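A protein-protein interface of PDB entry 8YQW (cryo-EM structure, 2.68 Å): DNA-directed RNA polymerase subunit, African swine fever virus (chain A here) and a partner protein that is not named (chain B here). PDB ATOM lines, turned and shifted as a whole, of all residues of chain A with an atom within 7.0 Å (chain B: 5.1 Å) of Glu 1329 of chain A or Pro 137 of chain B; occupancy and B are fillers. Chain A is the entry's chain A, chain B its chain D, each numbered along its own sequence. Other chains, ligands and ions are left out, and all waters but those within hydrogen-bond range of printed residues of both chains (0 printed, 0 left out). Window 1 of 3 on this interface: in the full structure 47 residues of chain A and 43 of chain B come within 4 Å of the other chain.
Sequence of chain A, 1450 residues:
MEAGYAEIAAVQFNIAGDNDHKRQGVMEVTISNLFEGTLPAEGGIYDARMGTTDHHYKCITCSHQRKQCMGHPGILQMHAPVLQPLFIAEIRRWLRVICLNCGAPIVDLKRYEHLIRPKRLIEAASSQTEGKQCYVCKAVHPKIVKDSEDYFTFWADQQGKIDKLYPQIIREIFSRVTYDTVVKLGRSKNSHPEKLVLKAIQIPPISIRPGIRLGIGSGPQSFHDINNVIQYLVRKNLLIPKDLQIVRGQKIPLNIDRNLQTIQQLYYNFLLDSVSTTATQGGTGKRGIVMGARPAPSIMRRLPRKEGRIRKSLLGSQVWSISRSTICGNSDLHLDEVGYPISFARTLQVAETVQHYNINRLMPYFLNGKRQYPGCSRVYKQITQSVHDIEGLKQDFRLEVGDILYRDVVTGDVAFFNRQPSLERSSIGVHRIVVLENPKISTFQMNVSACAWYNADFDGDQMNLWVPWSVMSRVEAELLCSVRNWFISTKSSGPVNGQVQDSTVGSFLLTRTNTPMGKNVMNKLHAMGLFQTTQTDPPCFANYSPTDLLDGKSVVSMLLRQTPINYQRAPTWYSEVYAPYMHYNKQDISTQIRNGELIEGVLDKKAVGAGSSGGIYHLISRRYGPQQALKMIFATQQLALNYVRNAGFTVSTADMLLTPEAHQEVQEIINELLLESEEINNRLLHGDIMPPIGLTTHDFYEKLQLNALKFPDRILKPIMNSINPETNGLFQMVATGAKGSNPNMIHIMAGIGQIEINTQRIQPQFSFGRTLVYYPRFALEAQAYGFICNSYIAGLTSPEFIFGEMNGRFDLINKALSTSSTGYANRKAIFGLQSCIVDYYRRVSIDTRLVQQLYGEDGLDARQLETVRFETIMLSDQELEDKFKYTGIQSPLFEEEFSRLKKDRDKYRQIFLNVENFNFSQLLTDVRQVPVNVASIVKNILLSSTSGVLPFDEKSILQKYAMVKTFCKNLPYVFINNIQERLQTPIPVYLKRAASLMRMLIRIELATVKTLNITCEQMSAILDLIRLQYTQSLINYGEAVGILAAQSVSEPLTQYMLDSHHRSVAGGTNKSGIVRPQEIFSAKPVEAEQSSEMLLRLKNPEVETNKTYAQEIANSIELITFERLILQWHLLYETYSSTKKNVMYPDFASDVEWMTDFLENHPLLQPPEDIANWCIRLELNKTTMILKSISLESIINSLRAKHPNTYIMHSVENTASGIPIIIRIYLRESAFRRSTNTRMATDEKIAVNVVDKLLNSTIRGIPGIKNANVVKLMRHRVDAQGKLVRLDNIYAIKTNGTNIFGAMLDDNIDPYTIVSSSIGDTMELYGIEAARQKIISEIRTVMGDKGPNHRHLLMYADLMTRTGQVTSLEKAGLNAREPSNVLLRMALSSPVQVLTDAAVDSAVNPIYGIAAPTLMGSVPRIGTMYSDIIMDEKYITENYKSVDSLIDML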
ATOM      1  N   ASN A 914     -15.146  24.585 -32.055  1.00  0.00           N
ATOM      2  CA  ASN A 914     -15.257  23.472 -31.119  1.00  0.00           C
ATOM      3  C   ASN A 914     -15.854  23.922 -29.793  1.00  0.00           C
ATOM      4  O   ASN A 914     -16.679  23.213 -29.208  1.00  0.00           O
ATOM      5  CB  ASN A 914     -13.884  22.842 -30.901  1.00  0.00           C
ATOM      6  CG  ASN A 914     -13.954  21.534 -30.146  1.00  0.00           C
ATOM      7  OD1 ASN A 914     -15.032  21.057 -29.802  1.00  0.00           O
ATOM      8  ND2 ASN A 914     -12.798  20.946 -29.880  1.00  0.00           N
ATOM      9  N   THR A1322     -21.231  14.403 -17.240  1.00  0.00           N
ATOM     10  CA  THR A1322     -20.114  14.647 -18.149  1.00  0.00           C
ATOM     11  C   THR A1322     -18.830  14.015 -17.629  1.00  0.00           C
ATOM     12  O   THR A1322     -18.041  13.467 -18.406  1.00  0.00           O
ATOM     13  CB  THR A1322     -19.924  16.150 -18.353  1.00  0.00           C
ATOM     14  OG1 THR A1322     -21.160  16.735 -18.781  1.00  0.00           O
ATOM     15  CG2 THR A1322     -18.857  16.419 -19.393  1.00  0.00           C
ATOM     16  N   MET A1323     -18.599  14.092 -16.318  1.00  0.00           N
ATOM     17  CA  MET A1323     -17.430  13.449 -15.730  1.00  0.00           C
ATOM     18  C   MET A1323     -17.511  11.934 -15.861  1.00  0.00           C
ATOM     19  O   MET A1323     -16.491  11.268 -16.077  1.00  0.00           O
ATOM     20  CB  MET A1323     -17.297  13.863 -14.265  1.00  0.00           C
ATOM     21  CG  MET A1323     -16.269  13.079 -13.474  1.00  0.00           C
ATOM     22  SD  MET A1323     -14.580  13.415 -13.991  1.00  0.00           S
ATOM     23  CE  MET A1323     -13.704  12.087 -13.179  1.00  0.00           C
ATOM     24  N   TYR A1326     -17.234  11.276 -20.092  1.00  0.00           N
ATOM     25  CA  TYR A1326     -16.212  11.921 -20.904  1.00  0.00           C
ATOM     26  C   TYR A1326     -14.858  12.009 -20.213  1.00  0.00           C
ATOM     27  O   TYR A1326     -13.837  11.717 -20.839  1.00  0.00           O
ATOM     28  CB  TYR A1326     -16.679  13.318 -21.316  1.00  0.00           C
ATOM     29  CG  TYR A1326     -17.864  13.310 -22.257  1.00  0.00           C
ATOM     30  CD1 TYR A1326     -18.045  12.282 -23.170  1.00  0.00           C
ATOM     31  CD2 TYR A1326     -18.802  14.330 -22.229  1.00  0.00           C
ATOM     32  CE1 TYR A1326     -19.124  12.270 -24.027  1.00  0.00           C
ATOM     33  CE2 TYR A1326     -19.884  14.326 -23.084  1.00  0.00           C
ATOM     34  CZ  TYR A1326     -20.040  13.295 -23.981  1.00  0.00           C
ATOM     35  OH  TYR A1326     -21.116  13.291 -24.835  1.00  0.00           O
ATOM     36  N   GLY A1327     -14.813  12.400 -18.944  1.00  0.00           N
ATOM     37  CA  GLY A1327     -13.572  12.418 -18.207  1.00  0.00           C
ATOM     38  C   GLY A1327     -13.398  13.701 -17.436  1.00  0.00           C
ATOM     39  O   GLY A1327     -14.288  14.554 -17.384  1.00  0.00           O
ATOM     40  N   ILE A1328     -12.224  13.839 -16.819  1.00  0.00           N
ATOM     41  CA  ILE A1328     -11.945  15.002 -15.983  1.00  0.00           C
ATOM     42  C   ILE A1328     -11.734  16.259 -16.821  1.00  0.00           C
ATOM     43  O   ILE A1328     -12.073  17.362 -16.380  1.00  0.00           O
ATOM     44  CB  ILE A1328     -10.744  14.723 -15.059  1.00  0.00           C
ATOM     45  CG1 ILE A1328     -10.703  15.738 -13.919  1.00  0.00           C
ATOM     46  CG2 ILE A1328      -9.433  14.736 -15.829  1.00  0.00           C
ATOM     47  CD1 ILE A1328     -11.949  15.752 -13.080  1.00  0.00           C
ATOM     48  N   GLU A1329     -11.177  16.131 -18.026  1.00  0.00           N
ATOM     49  CA  GLU A1329     -10.920  17.315 -18.837  1.00  0.00           C
ATOM     50  C   GLU A1329     -12.213  17.900 -19.385  1.00  0.00           C
ATOM     51  O   GLU A1329     -12.362  19.124 -19.464  1.00  0.00           O
ATOM     52  CB  GLU A1329      -9.957  16.979 -19.968  1.00  0.00           C
ATOM     53  CG  GLU A1329      -8.508  16.927 -19.537  1.00  0.00           C
ATOM     54  CD  GLU A1329      -8.001  18.268 -19.059  1.00  0.00           C
ATOM     55  OE1 GLU A1329      -8.435  19.300 -19.606  1.00  0.00           O
ATOM     56  OE2 GLU A1329      -7.169  18.293 -18.131  1.00  0.00           O
ATOM     57  N   ALA A1330     -13.157  17.045 -19.776  1.00  0.00           N
ATOM     58  CA  ALA A1330     -14.460  17.538 -20.200  1.00  0.00           C
ATOM     59  C   ALA A1330     -15.262  18.058 -19.017  1.00  0.00           C
ATOM     60  O   ALA A1330     -16.021  19.023 -19.151  1.00  0.00           O
ATOM     61  CB  ALA A1330     -15.225  16.440 -20.926  1.00  0.00           C
ATOM     62  N   ALA A1331     -15.114  17.424 -17.852  1.00  0.00           N
ATOM     63  CA  ALA A1331     -15.775  17.919 -16.652  1.00  0.00           C
ATOM     64  C   ALA A1331     -15.219  19.269 -16.228  1.00  0.00           C
ATOM     65  O   ALA A1331     -15.950  20.087 -15.663  1.00  0.00           O
ATOM     66  CB  ALA A1331     -15.634  16.910 -15.518  1.00  0.00           C
ATOM     67  N   ARG A1332     -13.933  19.512 -16.475  1.00  0.00           N
ATOM     68  CA  ARG A1332     -13.367  20.832 -16.225  1.00  0.00           C
ATOM     69  C   ARG A1332     -14.019  21.885 -17.111  1.00  0.00           C
ATOM     70  O   ARG A1332     -14.360  22.976 -16.644  1.00  0.00           O
ATOM     71  CB  ARG A1332     -11.858  20.798 -16.451  1.00  0.00           C
ATOM     72  CG  ARG A1332     -11.125  22.018 -15.944  1.00  0.00           C
ATOM     73  CD  ARG A1332      -9.766  22.137 -16.593  1.00  0.00           C
ATOM     74  NE  ARG A1332      -9.851  22.754 -17.910  1.00  0.00           N
ATOM     75  CZ  ARG A1332      -9.497  24.003 -18.177  1.00  0.00           C
ATOM     76  NH1 ARG A1332      -9.028  24.804 -17.235  1.00  0.00           N
ATOM     77  NH2 ARG A1332      -9.616  24.459 -19.419  1.00  0.00           N
ATOM     78  N   GLN A1333     -14.204  21.570 -18.394  1.00  0.00           N
ATOM     79  CA  GLN A1333     -14.891  22.486 -19.294  1.00  0.00           C
ATOM     80  C   GLN A1333     -16.363  22.635 -18.934  1.00  0.00           C
ATOM     81  O   GLN A1333     -16.977  23.655 -19.261  1.00  0.00           O
ATOM     82  CB  GLN A1333     -14.754  22.005 -20.735  1.00  0.00           C
ATOM     83  CG  GLN A1333     -13.386  22.215 -21.348  1.00  0.00           C
ATOM     84  CD  GLN A1333     -13.056  23.676 -21.561  1.00  0.00           C
ATOM     85  OE1 GLN A1333     -13.925  24.539 -21.489  1.00  0.00           O
ATOM     86  NE2 GLN A1333     -11.791  23.956 -21.836  1.00  0.00           N
ATOM     87  N   LYS A1334     -16.948  21.631 -18.282  1.00  0.00           N
ATOM     88  CA  LYS A1334     -18.353  21.710 -17.904  1.00  0.00           C
ATOM     89  C   LYS A1334     -18.560  22.614 -16.698  1.00  0.00           C
ATOM     90  O   LYS A1334     -19.566  23.325 -16.619  1.00  0.00           O
ATOM     91  CB  LYS A1334     -18.903  20.314 -17.622  1.00  0.00           C
ATOM     92  CG  LYS A1334     -20.410  20.261 -17.449  1.00  0.00           C
ATOM     93  CD  LYS A1334     -21.123  20.960 -18.586  1.00  0.00           C
ATOM     94  CE  LYS A1334     -20.818  20.302 -19.919  1.00  0.00           C
ATOM     95  NZ  LYS A1334     -21.420  21.067 -21.041  1.00  0.00           N
ATOM     96  N   ASP A1358     -10.139  24.439 -12.290  1.00  0.00           N
ATOM     97  CA  ASP A1358      -8.827  23.820 -12.137  1.00  0.00           C
ATOM     98  C   ASP A1358      -8.601  23.345 -10.710  1.00  0.00           C
ATOM     99  O   ASP A1358      -7.926  22.335 -10.486  1.00  0.00           O
ATOM    100  CB  ASP A1358      -7.738  24.803 -12.557  1.00  0.00           C
ATOM    101  CG  ASP A1358      -7.620  24.920 -14.058  1.00  0.00           C
ATOM    102  OD1 ASP A1358      -7.795  23.898 -14.748  1.00  0.00           O
ATOM    103  OD2 ASP A1358      -7.369  26.034 -14.554  1.00  0.00           O
ATOM    104  N   THR A1361     -10.911  20.092 -10.128  1.00  0.00           N
ATOM    105  CA  THR A1361     -10.563  18.922 -10.925  1.00  0.00           C
ATOM    106  C   THR A1361      -9.081  18.584 -10.823  1.00  0.00           C
ATOM    107  O   THR A1361      -8.554  17.876 -11.684  1.00  0.00           O
ATOM    108  CB  THR A1361     -10.945  19.135 -12.390  1.00  0.00           C
ATOM    109  OG1 THR A1361     -10.169  20.206 -12.934  1.00  0.00           O
ATOM    110  CG2 THR A1361     -12.417  19.478 -12.511  1.00  0.00           C
ATOM    111  N   ALA B 135     -16.223  17.583 -26.734  1.00  0.00           N
ATOM    112  CA  ALA B 135     -15.891  18.146 -25.432  1.00  0.00           C
ATOM    113  C   ALA B 135     -14.595  17.599 -24.855  1.00  0.00           C
ATOM    114  O   ALA B 135     -14.140  18.104 -23.824  1.00  0.00           O
ATOM    115  CB  ALA B 135     -17.030  17.895 -24.445  1.00  0.00           C
ATOM    116  N   ILE B 136     -13.997  16.591 -25.476  1.00  0.00           N
ATOM    117  CA  ILE B 136     -12.804  15.931 -24.953  1.00  0.00           C
ATOM    118  C   ILE B 136     -11.580  16.549 -25.621  1.00  0.00           C
ATOM    119  O   ILE B 136     -11.451  16.458 -26.852  1.00  0.00           O
ATOM    120  CB  ILE B 136     -12.859  14.415 -25.182  1.00  0.00           C
ATOM    121  CG1 ILE B 136     -13.859  13.787 -24.213  1.00  0.00           C
ATOM    122  CG2 ILE B 136     -11.490  13.793 -24.997  1.00  0.00           C
ATOM    123  CD1 ILE B 136     -14.162  12.355 -24.492  1.00  0.00           C
ATOM    124  N   PRO B 137     -10.669  17.177 -24.865  1.00  0.00           N
ATOM    125  CA  PRO B 137      -9.455  17.750 -25.467  1.00  0.00           C
ATOM    126  C   PRO B 137      -8.543  16.691 -26.058  1.00  0.00           C
ATOM    127  O   PRO B 137      -8.843  15.497 -25.970  1.00  0.00           O
ATOM    128  CB  PRO B 137      -8.782  18.464 -24.288  1.00  0.00           C
ATOM    129  CG  PRO B 137      -9.855  18.668 -23.294  1.00  0.00           C
ATOM    130  CD  PRO B 137     -10.798  17.526 -23.443  1.00  0.00           C
ATOM    131  N   LYS B 138      -7.426  17.095 -26.657  1.00  0.00           N
ATOM    132  CA  LYS B 138      -6.539  16.143 -27.316  1.00  0.00           C
ATOM    133  C   LYS B 138      -5.548  15.610 -26.288  1.00  0.00           C
ATOM    134  O   LYS B 138      -4.661  16.337 -25.837  1.00  0.00           O
ATOM    135  CB  LYS B 138      -5.820  16.793 -28.494  1.00  0.00           C
ATOM    136  CG  LYS B 138      -5.135  15.803 -29.425  1.00  0.00           C
ATOM    137  CD  LYS B 138      -3.673  15.577 -29.071  1.00  0.00           C
ATOM    138  CE  LYS B 138      -2.814  16.771 -29.435  1.00  0.00           C
ATOM    139  NZ  LYS B 138      -1.385  16.532 -29.106  1.00  0.00           N
ATOM    140  N   HIS B 139      -5.706  14.345 -25.910  1.00  0.00           N
ATOM    141  CA  HIS B 139      -4.784  13.684 -24.999  1.00  0.00           C
ATOM    142  C   HIS B 139      -3.685  12.985 -25.788  1.00  0.00           C
ATOM    143  O   HIS B 139      -3.885  12.571 -26.931  1.00  0.00           O
ATOM    144  CB  HIS B 139      -5.517  12.666 -24.125  1.00  0.00           C
ATOM    145  CG  HIS B 139      -6.502  13.271 -23.174  1.00  0.00           C
ATOM    146  ND1 HIS B 139      -7.583  14.015 -23.592  1.00  0.00           N
ATOM    147  CD2 HIS B 139      -6.580  13.220 -21.825  1.00  0.00           C
ATOM    148  CE1 HIS B 139      -8.277  14.407 -22.540  1.00  0.00           C
ATOM    149  NE2 HIS B 139      -7.691  13.938 -21.456  1.00  0.00           N
ATOM    150  N   ILE B 164      -4.487  12.395 -13.185  1.00  0.00           N
ATOM    151  CA  ILE B 164      -5.629  11.887 -13.932  1.00  0.00           C
ATOM    152  C   ILE B 164      -5.714  10.384 -13.711  1.00  0.00           C
ATOM    153  O   ILE B 164      -4.689   9.698 -13.647  1.00  0.00           O
ATOM    154  CB  ILE B 164      -5.513  12.235 -15.433  1.00  0.00           C
ATOM    155  CG1 ILE B 164      -6.797  11.886 -16.182  1.00  0.00           C
ATOM    156  CG2 ILE B 164      -4.311  11.555 -16.065  1.00  0.00           C
ATOM    157  CD1 ILE B 164      -6.950  12.634 -17.478  1.00  0.00           C
ATOM    158  N   ASP B 168      -9.896   7.020 -16.714  1.00  0.00           N
ATOM    159  CA  ASP B 168     -10.477   8.139 -17.440  1.00  0.00           C
ATOM    160  C   ASP B 168     -10.637   7.752 -18.907  1.00  0.00           C
ATOM    161  O   ASP B 168      -9.710   7.174 -19.490  1.00  0.00           O
ATOM    162  CB  ASP B 168      -9.584   9.370 -17.299  1.00  0.00           C
ATOM    163  CG  ASP B 168     -10.338  10.669 -17.481  1.00  0.00           C
ATOM    164  OD1 ASP B 168     -11.134  11.018 -16.588  1.00  0.00           O
ATOM    165  OD2 ASP B 168     -10.115  11.357 -18.499  1.00  0.00           O
ATOM    166  N   ILE B 184      -2.057  17.097 -22.456  1.00  0.00           N
ATOM    167  CA  ILE B 184      -3.387  17.454 -22.923  1.00  0.00           C
ATOM    168  C   ILE B 184      -3.309  18.822 -23.579  1.00  0.00           C
ATOM    169  O   ILE B 184      -2.928  19.809 -22.933  1.00  0.00           O
ATOM    170  CB  ILE B 184      -4.411  17.450 -21.780  1.00  0.00           C
ATOM    171  CG1 ILE B 184      -4.396  16.096 -21.073  1.00  0.00           C
ATOM    172  CG2 ILE B 184      -5.792  17.772 -22.310  1.00  0.00           C
ATOM    173  CD1 ILE B 184      -4.933  16.133 -19.675  1.00  0.00           C
ATOM    174  N   GLU B 185      -3.645  18.868 -24.864  1.00  0.00           N
ATOM    175  CA  GLU B 185      -3.852  20.105 -25.601  1.00  0.00           C
ATOM    176  C   GLU B 185      -5.329  20.460 -25.508  1.00  0.00           C
ATOM    177  O   GLU B 185      -6.178  19.727 -26.032  1.00  0.00           O
ATOM    178  CB  GLU B 185      -3.428  19.941 -27.059  1.00  0.00           C
ATOM    179  CG  GLU B 185      -3.750  21.129 -27.938  1.00  0.00           C
ATOM    180  CD  GLU B 185      -2.711  22.222 -27.847  1.00  0.00           C
ATOM    181  OE1 GLU B 185      -1.519  21.890 -27.693  1.00  0.00           O
ATOM    182  OE2 GLU B 185      -3.084  23.409 -27.928  1.00  0.00           O
ATOM    183  N   ARG B 186      -5.635  21.565 -24.837  1.00  0.00           N
ATOM    184  CA  ARG B 186      -7.026  21.888 -24.572  1.00  0.00           C
ATOM    185  C   ARG B 186      -7.355  23.306 -25.011  1.00  0.00           C
ATOM    186  O   ARG B 186      -6.501  24.193 -24.963  1.00  0.00           O
ATOM    187  CB  ARG B 186      -7.360  21.722 -23.082  1.00  0.00           C
ATOM    188  CG  ARG B 186      -6.495  22.510 -22.123  1.00  0.00           C
ATOM    189  CD  ARG B 186      -6.555  21.882 -20.743  1.00  0.00           C
ATOM    190  NE  ARG B 186      -6.217  22.816 -19.678  1.00  0.00           N
ATOM    191  CZ  ARG B 186      -6.149  22.492 -18.394  1.00  0.00           C
ATOM    192  NH1 ARG B 186      -6.394  21.262 -17.977  1.00  0.00           N
ATOM    193  NH2 ARG B 186      -5.823  23.426 -17.506  1.00  0.00           N
ATOM    194  N   PRO B 187      -8.590  23.540 -25.453  1.00  0.00           N
ATOM    195  CA  PRO B 187      -8.981  24.889 -25.872  1.00  0.00           C
ATOM    196  C   PRO B 187      -9.024  25.853 -24.700  1.00  0.00           C
ATOM    197  O   PRO B 187      -9.265  25.471 -23.553  1.00  0.00           O
ATOM    198  CB  PRO B 187     -10.378  24.685 -26.470  1.00  0.00           C
ATOM    199  CG  PRO B 187     -10.494  23.228 -26.714  1.00  0.00           C
ATOM    200  CD  PRO B 187      -9.671  22.567 -25.667  1.00  0.00           C
ATOM    201  N   VAL B 196      -1.284  21.187 -20.873  1.00  0.00           N
ATOM    202  CA  VAL B 196      -1.017  20.734 -19.516  1.00  0.00           C
ATOM    203  C   VAL B 196      -0.441  19.328 -19.579  1.00  0.00           C
ATOM    204  O   VAL B 196      -0.558  18.631 -20.584  1.00  0.00           O
ATOM    205  CB  VAL B 196      -2.267  20.765 -18.614  1.00  0.00           C
ATOM    206  CG1 VAL B 196      -2.663  22.196 -18.318  1.00  0.00           C
ATOM    207  CG2 VAL B 196      -3.407  20.011 -19.263  1.00  0.00           C
ATOM    208  N   ARG B 198      -0.331  15.816 -17.146  1.00  0.00           N
ATOM    209  CA  ARG B 198      -0.961  15.169 -16.011  1.00  0.00           C
ATOM    210  C   ARG B 198      -0.283  13.838 -15.724  1.00  0.00           C
ATOM    211  O   ARG B 198       0.231  13.174 -16.629  1.00  0.00           O
ATOM    212  CB  ARG B 198      -2.456  14.950 -16.256  1.00  0.00           C
ATOM    213  CG  ARG B 198      -3.299  16.196 -16.081  1.00  0.00           C
ATOM    214  CD  ARG B 198      -4.768  15.854 -16.023  1.00  0.00           C
ATOM    215  NE  ARG B 198      -5.590  17.025 -15.753  1.00  0.00           N
ATOM    216  CZ  ARG B 198      -6.249  17.236 -14.624  1.00  0.00           C
ATOM    217  NH1 ARG B 198      -6.212  16.368 -13.629  1.00  0.00           N
ATOM    218  NH2 ARG B 198      -6.965  18.348 -14.490  1.00  0.00           N
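The backbone NH of Ile 1328 of chain A lies within hydrogen-bond range of the side-chain carboxylate of Asp 168 of chain B (3.0 Å).
The side-chain carboxylate of Glu 1329 of chain A is in salt-bridge range of the guanidinium group of Arg 186 of chain B, at 3.1 Å.
OE2 of Glu 1329 of chain A lies within salt-bridge range of NE of Arg 198 of chain B (3.1 Å).
The side-chain amide nitrogen (NE2) of Gln 1333 of chain A lies within hydrogen-bond range of the backbone carbonyl oxygen (O) of Pro 187 of chain B, at 3.4 Å.
NH2 of Arg 186 of chain B is in salt-bridge range of OD1 of Asp 1358 of chain A.
The backbone carbonyl oxygen of Thr 1361 of chain A sits at hydrogen-bond distance from the guanidinium group of Arg 198 of chain B, 3.3 Å away.
The guanidinium group (NH1) of Arg 1332 of chain A lies close to the guanidinium group (NH2) of Arg 186 of chain B.
The backbone carbonyl oxygen (O) of Thr 1322 of chain A is in hydrogen-bond range of the backbone NH (N) of Gly 1327 of chain A (3.4 Å).
The side-chain sulfur (SD) of Met 1323 of chain A lies close to the backbone NH (N) of Ile 1328 of chain A.
NH2 of Arg 1332 of chain A lies close to NE2 of Gln 1333 of chain A (3.3 Å).
The guanidinium group of Arg 1332 of chain A is in salt-bridge range of the side-chain carboxylate of Asp 1358 of chain A (2.9 Å).
A ring nitrogen (ND1) of His 139 of chain B lies within hydrogen-bond range of the backbone carbonyl oxygen (O) of Pro 137 of chain B, 3.1 Å away.
O of Val 196 of chain B sits at hydrogen-bond distance from N of Ile 184 of chain B.
Among the printed residues, pairs that only touch across the chains: Gly 1327 of chain A with Asp 168 of chain B (3.2 Å), Glu 1329 of chain A with Ile 184 of chain B (3.5 Å), Ala 1330 of chain A with Ala 135 of chain B (3.5 Å), Glu 1329 of chain A with Pro 137 of chain B (3.6 Å), Glu 1329 of chain A with His 139 of chain B (3.6 Å), Ile 1328 of chain A with Ile 164 of chain B (3.6 Å) and Tyr 1326 of chain A with Ile 136 of chain B (3.7 Å).
Of the printed residues of chain B, Gly 1327 of chain A touches Asp 168 (3.2 Å).
Glu 1329 of chain A touches five residues of chain B.
Of the printed residues of chain A, Ala 135 of chain B touches Ala 1330.
Pro 137 of chain B touches just one residue of chain A: Glu 1329 (3.6 Å).
Of the printed residues of chain A, Ile 184 of chain B touches Glu 1329 (3.5 Å).
The nearest residue of chain A that does not touch Pro 137 of chain B is Ala 1330 of chain A (4.4 Å).
Of the 14 printed residues of chain A, 9 touch a printed residue of chain B.
Hydrophobic or aromatic side chains of chain B that line the printed part of chain A: Ile 136, Pro 137, His 139, Ile 164 and Ile 184.
Among the printed residues, Asp or Glu carboxylates within 4 Å of a Lys or Arg side-chain nitrogen of the other chain: Glu 1329 of chain A with Arg 186 of chain B, Glu 1329 of chain A with Arg 198 of chain B and Asp 1358 of chain A with Arg 186 of chain B.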
